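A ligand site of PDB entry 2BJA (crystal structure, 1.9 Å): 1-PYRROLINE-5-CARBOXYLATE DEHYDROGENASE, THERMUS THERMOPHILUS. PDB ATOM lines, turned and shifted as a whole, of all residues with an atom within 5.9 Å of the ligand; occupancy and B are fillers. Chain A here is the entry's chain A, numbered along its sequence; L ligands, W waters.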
ATOM      1  N   ILE A 180     -21.387  -7.523  19.321  1.00  0.00           N
ATOM      2  CA  ILE A 180     -22.202  -6.972  20.389  1.00  0.00           C
ATOM      3  C   ILE A 180     -22.313  -8.048  21.457  1.00  0.00           C
ATOM      4  O   ILE A 180     -23.030  -9.037  21.268  1.00  0.00           O
ATOM      5  CB  ILE A 180     -23.586  -6.579  19.852  1.00  0.00           C
ATOM      6  CG1 ILE A 180     -23.397  -5.478  18.794  1.00  0.00           C
ATOM      7  CG2 ILE A 180     -24.471  -6.100  20.968  1.00  0.00           C
ATOM      8  CD1 ILE A 180     -24.682  -5.055  18.074  1.00  0.00           C
ATOM      9  N   ALA A 181     -21.595  -7.835  22.555  1.00  0.00           N
ATOM     10  CA  ALA A 181     -21.493  -8.798  23.651  1.00  0.00           C
ATOM     11  C   ALA A 181     -22.386  -8.637  24.879  1.00  0.00           C
ATOM     12  O   ALA A 181     -22.924  -7.562  25.151  1.00  0.00           O
ATOM     13  CB  ALA A 181     -20.025  -8.875  24.104  1.00  0.00           C
ATOM     14  N   PRO A 182     -22.545  -9.715  25.657  1.00  0.00           N
ATOM     15  CA  PRO A 182     -23.366  -9.716  26.857  1.00  0.00           C
ATOM     16  C   PRO A 182     -22.544  -9.389  28.098  1.00  0.00           C
ATOM     17  O   PRO A 182     -21.314  -9.367  28.043  1.00  0.00           O
ATOM     18  CB  PRO A 182     -23.909 -11.130  26.884  1.00  0.00           C
ATOM     19  CG  PRO A 182     -22.689 -11.926  26.490  1.00  0.00           C
ATOM     20  CD  PRO A 182     -22.066 -11.088  25.357  1.00  0.00           C
ATOM     21  N   TRP A 183     -23.215  -9.148  29.224  1.00  0.00           N
ATOM     22  CA  TRP A 183     -22.505  -8.837  30.450  1.00  0.00           C
ATOM     23  C   TRP A 183     -22.183 -10.047  31.327  1.00  0.00           C
ATOM     24  O   TRP A 183     -21.342  -9.941  32.221  1.00  0.00           O
ATOM     25  CB  TRP A 183     -23.289  -7.820  31.293  1.00  0.00           C
ATOM     26  CG  TRP A 183     -24.720  -8.216  31.541  1.00  0.00           C
ATOM     27  CD1 TRP A 183     -25.811  -7.762  30.869  1.00  0.00           C
ATOM     28  CD2 TRP A 183     -25.205  -9.161  32.508  1.00  0.00           C
ATOM     29  NE1 TRP A 183     -26.954  -8.372  31.344  1.00  0.00           N
ATOM     30  CE2 TRP A 183     -26.612  -9.240  32.352  1.00  0.00           C
ATOM     31  CE3 TRP A 183     -24.599  -9.952  33.489  1.00  0.00           C
ATOM     32  CZ2 TRP A 183     -27.418 -10.076  33.129  1.00  0.00           C
ATOM     33  CZ3 TRP A 183     -25.399 -10.796  34.266  1.00  0.00           C
ATOM     34  CH2 TRP A 183     -26.793 -10.839  34.079  1.00  0.00           C
ATOM     35  N   LYS A 207     -18.646  -3.907  20.738  1.00  0.00           N
ATOM     36  CA  LYS A 207     -19.525  -3.124  21.601  1.00  0.00           C
ATOM     37  C   LYS A 207     -19.840  -3.913  22.879  1.00  0.00           C
ATOM     38  O   LYS A 207     -20.748  -4.747  22.888  1.00  0.00           O
ATOM     39  CB  LYS A 207     -20.820  -2.801  20.850  1.00  0.00           C
ATOM     40  CG  LYS A 207     -21.464  -1.462  21.211  1.00  0.00           C
ATOM     41  CD  LYS A 207     -21.840  -1.377  22.686  1.00  0.00           C
ATOM     42  CE  LYS A 207     -23.088  -2.179  22.990  1.00  0.00           C
ATOM     43  NZ  LYS A 207     -23.457  -2.024  24.420  1.00  0.00           N
ATOM     44  N   PRO A 208     -19.092  -3.676  23.965  1.00  0.00           N
ATOM     45  CA  PRO A 208     -19.316  -4.389  25.220  1.00  0.00           C
ATOM     46  C   PRO A 208     -20.622  -4.002  25.892  1.00  0.00           C
ATOM     47  O   PRO A 208     -21.156  -2.912  25.652  1.00  0.00           O
ATOM     48  CB  PRO A 208     -18.112  -3.993  26.068  1.00  0.00           C
ATOM     49  CG  PRO A 208     -17.899  -2.582  25.644  1.00  0.00           C
ATOM     50  CD  PRO A 208     -18.010  -2.683  24.129  1.00  0.00           C
ATOM     51  N   ALA A 209     -21.143  -4.899  26.724  1.00  0.00           N
ATOM     52  CA  ALA A 209     -22.383  -4.640  27.436  1.00  0.00           C
ATOM     53  C   ALA A 209     -22.167  -3.505  28.442  1.00  0.00           C
ATOM     54  O   ALA A 209     -21.079  -3.364  29.017  1.00  0.00           O
ATOM     55  CB  ALA A 209     -22.833  -5.895  28.162  1.00  0.00           C
ATOM     56  N   GLU A 210     -23.206  -2.704  28.640  1.00  0.00           N
ATOM     57  CA  GLU A 210     -23.158  -1.565  29.566  1.00  0.00           C
ATOM     58  C   GLU A 210     -22.601  -1.875  30.958  1.00  0.00           C
ATOM     59  O   GLU A 210     -21.804  -1.105  31.502  1.00  0.00           O
ATOM     60  CB  GLU A 210     -24.561  -0.950  29.709  1.00  0.00           C
ATOM     61  CG  GLU A 210     -25.071  -0.184  28.485  1.00  0.00           C
ATOM     62  CD  GLU A 210     -25.727  -1.074  27.424  1.00  0.00           C
ATOM     63  OE1 GLU A 210     -26.433  -0.521  26.549  1.00  0.00           O
ATOM     64  OE2 GLU A 210     -25.556  -2.310  27.445  1.00  0.00           O
ATOM     65  N   GLY A 238     -20.827   1.689  24.815  1.00  0.00           N
ATOM     66  CA  GLY A 238     -21.920   2.614  24.588  1.00  0.00           C
ATOM     67  C   GLY A 238     -23.257   1.918  24.777  1.00  0.00           C
ATOM     68  O   GLY A 238     -23.296   0.756  25.171  1.00  0.00           O
ATOM     69  N   VAL A 239     -24.333   2.634  24.490  1.00  0.00           N
ATOM     70  CA  VAL A 239     -25.682   2.085  24.645  1.00  0.00           C
ATOM     71  C   VAL A 239     -26.049   1.226  23.445  1.00  0.00           C
ATOM     72  O   VAL A 239     -25.985   1.677  22.302  1.00  0.00           O
ATOM     73  CB  VAL A 239     -26.726   3.220  24.815  1.00  0.00           C
ATOM     74  CG1 VAL A 239     -28.120   2.633  24.944  1.00  0.00           C
ATOM     75  CG2 VAL A 239     -26.383   4.045  26.057  1.00  0.00           C
ATOM     76  N   GLY A 240     -26.445  -0.013  23.720  1.00  0.00           N
ATOM     77  CA  GLY A 240     -26.814  -0.950  22.670  1.00  0.00           C
ATOM     78  C   GLY A 240     -27.835  -0.426  21.680  1.00  0.00           C
ATOM     79  O   GLY A 240     -27.577  -0.426  20.484  1.00  0.00           O
ATOM     80  N   GLU A 241     -28.987   0.023  22.173  1.00  0.00           N
ATOM     81  CA  GLU A 241     -30.055   0.548  21.317  1.00  0.00           C
ATOM     82  C   GLU A 241     -29.655   1.800  20.561  1.00  0.00           C
ATOM     83  O   GLU A 241     -30.441   2.300  19.754  1.00  0.00           O
ATOM     84  CB  GLU A 241     -31.340   0.823  22.130  1.00  0.00           C
ATOM     85  CG  GLU A 241     -31.154   1.414  23.520  1.00  0.00           C
ATOM     86  CD  GLU A 241     -30.907   0.311  24.549  1.00  0.00           C
ATOM     87  OE1 GLU A 241     -29.758  -0.151  24.650  1.00  0.00           O
ATOM     88  OE2 GLU A 241     -31.862  -0.103  25.250  1.00  0.00           O
ATOM     89  N   GLU A 242     -28.472   2.331  20.839  1.00  0.00           N
ATOM     90  CA  GLU A 242     -28.007   3.521  20.153  1.00  0.00           C
ATOM     91  C   GLU A 242     -26.881   3.192  19.187  1.00  0.00           C
ATOM     92  O   GLU A 242     -27.127   2.928  18.010  1.00  0.00           O
ATOM     93  CB  GLU A 242     -27.575   4.589  21.156  1.00  0.00           C
ATOM     94  CG  GLU A 242     -28.724   5.120  21.998  1.00  0.00           C
ATOM     95  CD  GLU A 242     -28.308   6.122  23.068  1.00  0.00           C
ATOM     96  OE1 GLU A 242     -29.168   6.491  23.888  1.00  0.00           O
ATOM     97  OE2 GLU A 242     -27.130   6.557  23.073  1.00  0.00           O
ATOM     98  N   GLY A 244     -25.122   0.517  19.102  1.00  0.00           N
ATOM     99  CA  GLY A 244     -25.194  -0.872  18.694  1.00  0.00           C
ATOM    100  C   GLY A 244     -26.138  -1.014  17.506  1.00  0.00           C
ATOM    101  O   GLY A 244     -25.767  -1.569  16.470  1.00  0.00           O
ATOM    102  N   ALA A 245     -27.356  -0.504  17.660  1.00  0.00           N
ATOM    103  CA  ALA A 245     -28.343  -0.563  16.581  1.00  0.00           C
ATOM    104  C   ALA A 245     -27.834   0.153  15.339  1.00  0.00           C
ATOM    105  O   ALA A 245     -28.034  -0.319  14.221  1.00  0.00           O
ATOM    106  CB  ALA A 245     -29.662   0.058  17.048  1.00  0.00           C
ATOM    107  N   VAL A 248     -25.559  -2.179  13.506  1.00  0.00           N
ATOM    108  CA  VAL A 248     -26.303  -3.295  12.951  1.00  0.00           C
ATOM    109  C   VAL A 248     -27.039  -2.939  11.651  1.00  0.00           C
ATOM    110  O   VAL A 248     -27.075  -3.716  10.699  1.00  0.00           O
ATOM    111  CB  VAL A 248     -27.326  -3.842  13.981  1.00  0.00           C
ATOM    112  CG1 VAL A 248     -28.335  -4.751  13.278  1.00  0.00           C
ATOM    113  CG2 VAL A 248     -26.595  -4.620  15.078  1.00  0.00           C
ATOM    114  N   PHE A 258     -23.464 -11.564  17.571  1.00  0.00           N
ATOM    115  CA  PHE A 258     -24.201 -11.170  18.755  1.00  0.00           C
ATOM    116  C   PHE A 258     -24.561 -12.284  19.716  1.00  0.00           C
ATOM    117  O   PHE A 258     -24.950 -13.377  19.300  1.00  0.00           O
ATOM    118  CB  PHE A 258     -25.508 -10.477  18.334  1.00  0.00           C
ATOM    119  CG  PHE A 258     -26.487 -10.258  19.455  1.00  0.00           C
ATOM    120  CD1 PHE A 258     -26.402  -9.129  20.271  1.00  0.00           C
ATOM    121  CD2 PHE A 258     -27.505 -11.182  19.701  1.00  0.00           C
ATOM    122  CE1 PHE A 258     -27.303  -8.911  21.304  1.00  0.00           C
ATOM    123  CE2 PHE A 258     -28.415 -10.985  20.739  1.00  0.00           C
ATOM    124  CZ  PHE A 258     -28.325  -9.851  21.543  1.00  0.00           C
ATOM    125  N   THR A 259     -24.448 -11.975  21.006  1.00  0.00           N
ATOM    126  CA  THR A 259     -24.817 -12.888  22.069  1.00  0.00           C
ATOM    127  C   THR A 259     -25.578 -12.032  23.091  1.00  0.00           C
ATOM    128  O   THR A 259     -25.095 -10.991  23.539  1.00  0.00           O
ATOM    129  CB  THR A 259     -23.582 -13.548  22.706  1.00  0.00           C
ATOM    130  OG1 THR A 259     -22.885 -14.313  21.712  1.00  0.00           O
ATOM    131  CG2 THR A 259     -23.989 -14.466  23.839  1.00  0.00           C
ATOM    132  N   GLY A 260     -26.791 -12.454  23.433  1.00  0.00           N
ATOM    133  CA  GLY A 260     -27.591 -11.698  24.378  1.00  0.00           C
ATOM    134  C   GLY A 260     -29.026 -12.202  24.439  1.00  0.00           C
ATOM    135  O   GLY A 260     -29.287 -13.383  24.209  1.00  0.00           O
ATOM    136  N   SER A 261     -29.952 -11.293  24.750  1.00  0.00           N
ATOM    137  CA  SER A 261     -31.362 -11.672  24.866  1.00  0.00           C
ATOM    138  C   SER A 261     -32.027 -11.999  23.539  1.00  0.00           C
ATOM    139  O   SER A 261     -31.617 -11.520  22.485  1.00  0.00           O
ATOM    140  CB  SER A 261     -32.158 -10.549  25.546  1.00  0.00           C
ATOM    141  OG  SER A 261     -32.257  -9.439  24.682  1.00  0.00           O
ATOM    142  N   LEU A 262     -33.086 -12.802  23.616  1.00  0.00           N
ATOM    143  CA  LEU A 262     -33.833 -13.195  22.433  1.00  0.00           C
ATOM    144  C   LEU A 262     -34.519 -11.961  21.836  1.00  0.00           C
ATOM    145  O   LEU A 262     -34.637 -11.831  20.613  1.00  0.00           O
ATOM    146  CB  LEU A 262     -34.876 -14.257  22.782  1.00  0.00           C
ATOM    147  CG  LEU A 262     -35.846 -14.615  21.660  1.00  0.00           C
ATOM    148  CD1 LEU A 262     -35.077 -15.217  20.496  1.00  0.00           C
ATOM    149  CD2 LEU A 262     -36.892 -15.587  22.169  1.00  0.00           C
ATOM    150  N   GLU A 263     -34.972 -11.072  22.705  1.00  0.00           N
ATOM    151  CA  GLU A 263     -35.648  -9.854  22.253  1.00  0.00           C
ATOM    152  C   GLU A 263     -34.765  -9.033  21.318  1.00  0.00           C
ATOM    153  O   GLU A 263     -35.192  -8.626  20.245  1.00  0.00           O
ATOM    154  CB  GLU A 263     -36.063  -8.996  23.452  1.00  0.00           C
ATOM    155  CG  GLU A 263     -36.299  -7.542  23.115  1.00  0.00           C
ATOM    156  CD  GLU A 263     -36.936  -6.765  24.261  1.00  0.00           C
ATOM    157  OE1 GLU A 263     -36.435  -6.875  25.400  1.00  0.00           O
ATOM    158  OE2 GLU A 263     -37.934  -6.062  24.012  1.00  0.00           O
ATOM    159  N   VAL A 264     -33.516  -8.798  21.729  1.00  0.00           N
ATOM    160  CA  VAL A 264     -32.587  -8.028  20.917  1.00  0.00           C
ATOM    161  C   VAL A 264     -32.117  -8.841  19.709  1.00  0.00           C
ATOM    162  O   VAL A 264     -31.988  -8.323  18.603  1.00  0.00           O
ATOM    163  CB  VAL A 264     -31.353  -7.569  21.768  1.00  0.00           C
ATOM    164  CG1 VAL A 264     -30.292  -6.964  20.865  1.00  0.00           C
ATOM    165  CG2 VAL A 264     -31.794  -6.539  22.806  1.00  0.00           C
ATOM    166  N   GLY A 265     -31.872 -10.132  19.922  1.00  0.00           N
ATOM    167  CA  GLY A 265     -31.435 -10.985  18.832  1.00  0.00           C
ATOM    168  C   GLY A 265     -32.425 -11.021  17.687  1.00  0.00           C
ATOM    169  O   GLY A 265     -32.032 -11.077  16.515  1.00  0.00           O
ATOM    170  N   LYS A 267     -34.473  -8.631  16.836  1.00  0.00           N
ATOM    171  CA  LYS A 267     -34.409  -7.332  16.152  1.00  0.00           C
ATOM    172  C   LYS A 267     -33.201  -7.269  15.233  1.00  0.00           C
ATOM    173  O   LYS A 267     -33.276  -6.752  14.118  1.00  0.00           O
ATOM    174  CB  LYS A 267     -34.308  -6.177  17.147  1.00  0.00           C
ATOM    175  CG  LYS A 267     -35.585  -5.857  17.898  1.00  0.00           C
ATOM    176  CD  LYS A 267     -35.423  -4.547  18.634  1.00  0.00           C
ATOM    177  CE  LYS A 267     -36.618  -4.222  19.512  1.00  0.00           C
ATOM    178  NZ  LYS A 267     -36.665  -5.088  20.715  1.00  0.00           N
ATOM    179  N   ILE A 268     -32.066  -7.779  15.709  1.00  0.00           N
ATOM    180  CA  ILE A 268     -30.836  -7.774  14.941  1.00  0.00           C
ATOM    181  C   ILE A 268     -30.936  -8.644  13.708  1.00  0.00           C
ATOM    182  O   ILE A 268     -30.541  -8.243  12.618  1.00  0.00           O
ATOM    183  CB  ILE A 268     -29.650  -8.239  15.813  1.00  0.00           C
ATOM    184  CG1 ILE A 268     -29.358  -7.171  16.877  1.00  0.00           C
ATOM    185  CG2 ILE A 268     -28.418  -8.506  14.948  1.00  0.00           C
ATOM    186  CD1 ILE A 268     -28.242  -7.564  17.834  1.00  0.00           C
HETATM  187  P1  LIG L   1     -29.287  -7.506  26.002  1.00  0.00           P
HETATM  188  O1  LIG L   1     -28.855  -8.102  27.326  1.00  0.00           O
HETATM  189  O2  LIG L   1     -29.787  -8.525  25.035  1.00  0.00           O
HETATM  190  O3  LIG L   1     -28.043  -6.774  25.338  1.00  0.00           O
HETATM  191  C1  LIG L   1     -26.844  -7.560  25.020  1.00  0.00           C
HETATM  192  C2  LIG L   1     -25.838  -6.634  24.331  1.00  0.00           C
HETATM  193  O4  LIG L   1     -26.492  -6.066  23.151  1.00  0.00           O
HETATM  194  C3  LIG L   1     -25.283  -5.400  25.122  1.00  0.00           C
HETATM  195  O5  LIG L   1     -24.007  -5.109  24.542  1.00  0.00           O
HETATM  196  C4  LIG L   1     -26.303  -4.313  24.757  1.00  0.00           C
HETATM  197  O6  LIG L   1     -25.813  -2.993  24.893  1.00  0.00           O
HETATM  198  C5  LIG L   1     -26.628  -4.656  23.289  1.00  0.00           C
HETATM  199  N1  LIG L   1     -27.965  -4.198  22.844  1.00  0.00           N
HETATM  200  C6  LIG L   1     -29.114  -3.979  23.565  1.00  0.00           C
HETATM  201  N2  LIG L   1     -30.147  -3.567  22.847  1.00  0.00           N
HETATM  202  C7  LIG L   1     -29.648  -3.523  21.562  1.00  0.00           C
HETATM  203  C8  LIG L   1     -30.225  -3.164  20.300  1.00  0.00           C
HETATM  204  N3  LIG L   1     -31.481  -2.766  20.129  1.00  0.00           N
HETATM  205  N4  LIG L   1     -29.417  -3.239  19.189  1.00  0.00           N
HETATM  206  C9  LIG L   1     -28.120  -3.643  19.311  1.00  0.00           C
HETATM  207  N5  LIG L   1     -27.474  -3.996  20.442  1.00  0.00           N
HETATM  208  C10 LIG L   1     -28.292  -3.917  21.534  1.00  0.00           C
HETATM  209  O7  LIG L   1     -30.363  -6.332  26.172  1.00  0.00           O
HETATM  210  P2  LIG L   1     -30.965  -5.681  27.499  1.00  0.00           P
HETATM  211  O8  LIG L   1     -30.063  -4.589  27.953  1.00  0.00           O
HETATM  212  O9  LIG L   1     -31.299  -6.813  28.417  1.00  0.00           O
HETATM  213  O10 LIG L   1     -32.348  -5.118  26.942  1.00  0.00           O
HETATM  214  O   HOH W   1     -33.871  -2.771  21.536  1.00  0.00           O
HETATM  215  O   HOH W   2     -29.214  -1.639  26.474  1.00  0.00           O
HETATM  216  O   HOH W   3     -26.291  -8.917  28.034  1.00  0.00           O
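Water W3 lies within hydrogen-bond range of an oxygen (O1) of the ligand and the backbone NH of Trp 183.
Water W2 lies within hydrogen-bond range of the side-chain carboxylate (OE1) of Glu 241, the side-chain carboxylate (OE1) of Glu 210 and an oxygen (O8) of the ligand.
The backbone NH (N) of Gly 240 lies close to an oxygen (O6) of the ligand, 3.3 Å away.
The backbone NH (N) of Ser 261 sits at hydrogen-bond distance from an oxygen (O2) of the ligand, 2.8 Å away.
The backbone carbonyl oxygen (O) of Ala 181 sits at hydrogen-bond distance from an oxygen (O5) of the ligand (2.7 Å).
An oxygen (O2) of the ligand sits at hydrogen-bond distance from the side-chain hydroxyl (OG) of Ser 261.
OE2 of Glu 210 sits at hydrogen-bond distance from O6 of the ligand, at 2.7 Å.
The side-chain amino group of Lys 207 lies within hydrogen-bond range of an oxygen (O6) of the ligand, at 2.6 Å.
Merely in contact with the ligand: Ile 180 (3.0 Å), Pro 208 (3.8 Å), Ala 209 (3.4 Å), Glu 241 (3.7 Å), Gly 244 (3.8 Å), Ala 245 (3.6 Å), Phe 258 (3.5 Å), Gly 260 (3.8 Å) and Val 264 (3.4 Å).
Hydrophobic or aromatic side chains that line the ligand: Ile 180, Ala 209, Ala 245, Phe 258 and Val 264.
14 residues have an atom within 4 Å of the ligand: Ile 180, Ala 181, Lys 207, Pro 208, Ala 209, Glu 210, Gly 240, Glu 241, Gly 244, Ala 245, Phe 258, Gly 260, Ser 261 and Val 264.
The backbone carbonyl oxygen (O) of Ile 180 sits at hydrogen-bond distance from the backbone NH (N) of Thr 259 (3.3 Å).
The side-chain carboxylate of Glu 210 lies within hydrogen-bond range of the backbone NH of Gly 240, at 2.9 Å.
OE2 of Glu 210 is in salt-bridge range of NZ of Lys 207, at 3.7 Å.
N of Val 264 sits at hydrogen-bond distance from OG of Ser 261.
The backbone NH (N) of Ala 245 sits at hydrogen-bond distance from the backbone carbonyl oxygen (O) of Gly 240.
The side-chain amino group of Lys 207 sits at hydrogen-bond distance from the backbone carbonyl oxygen of Gly 238 (2.9 Å).
O of Lys 207 lies within hydrogen-bond range of N of Ala 181.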
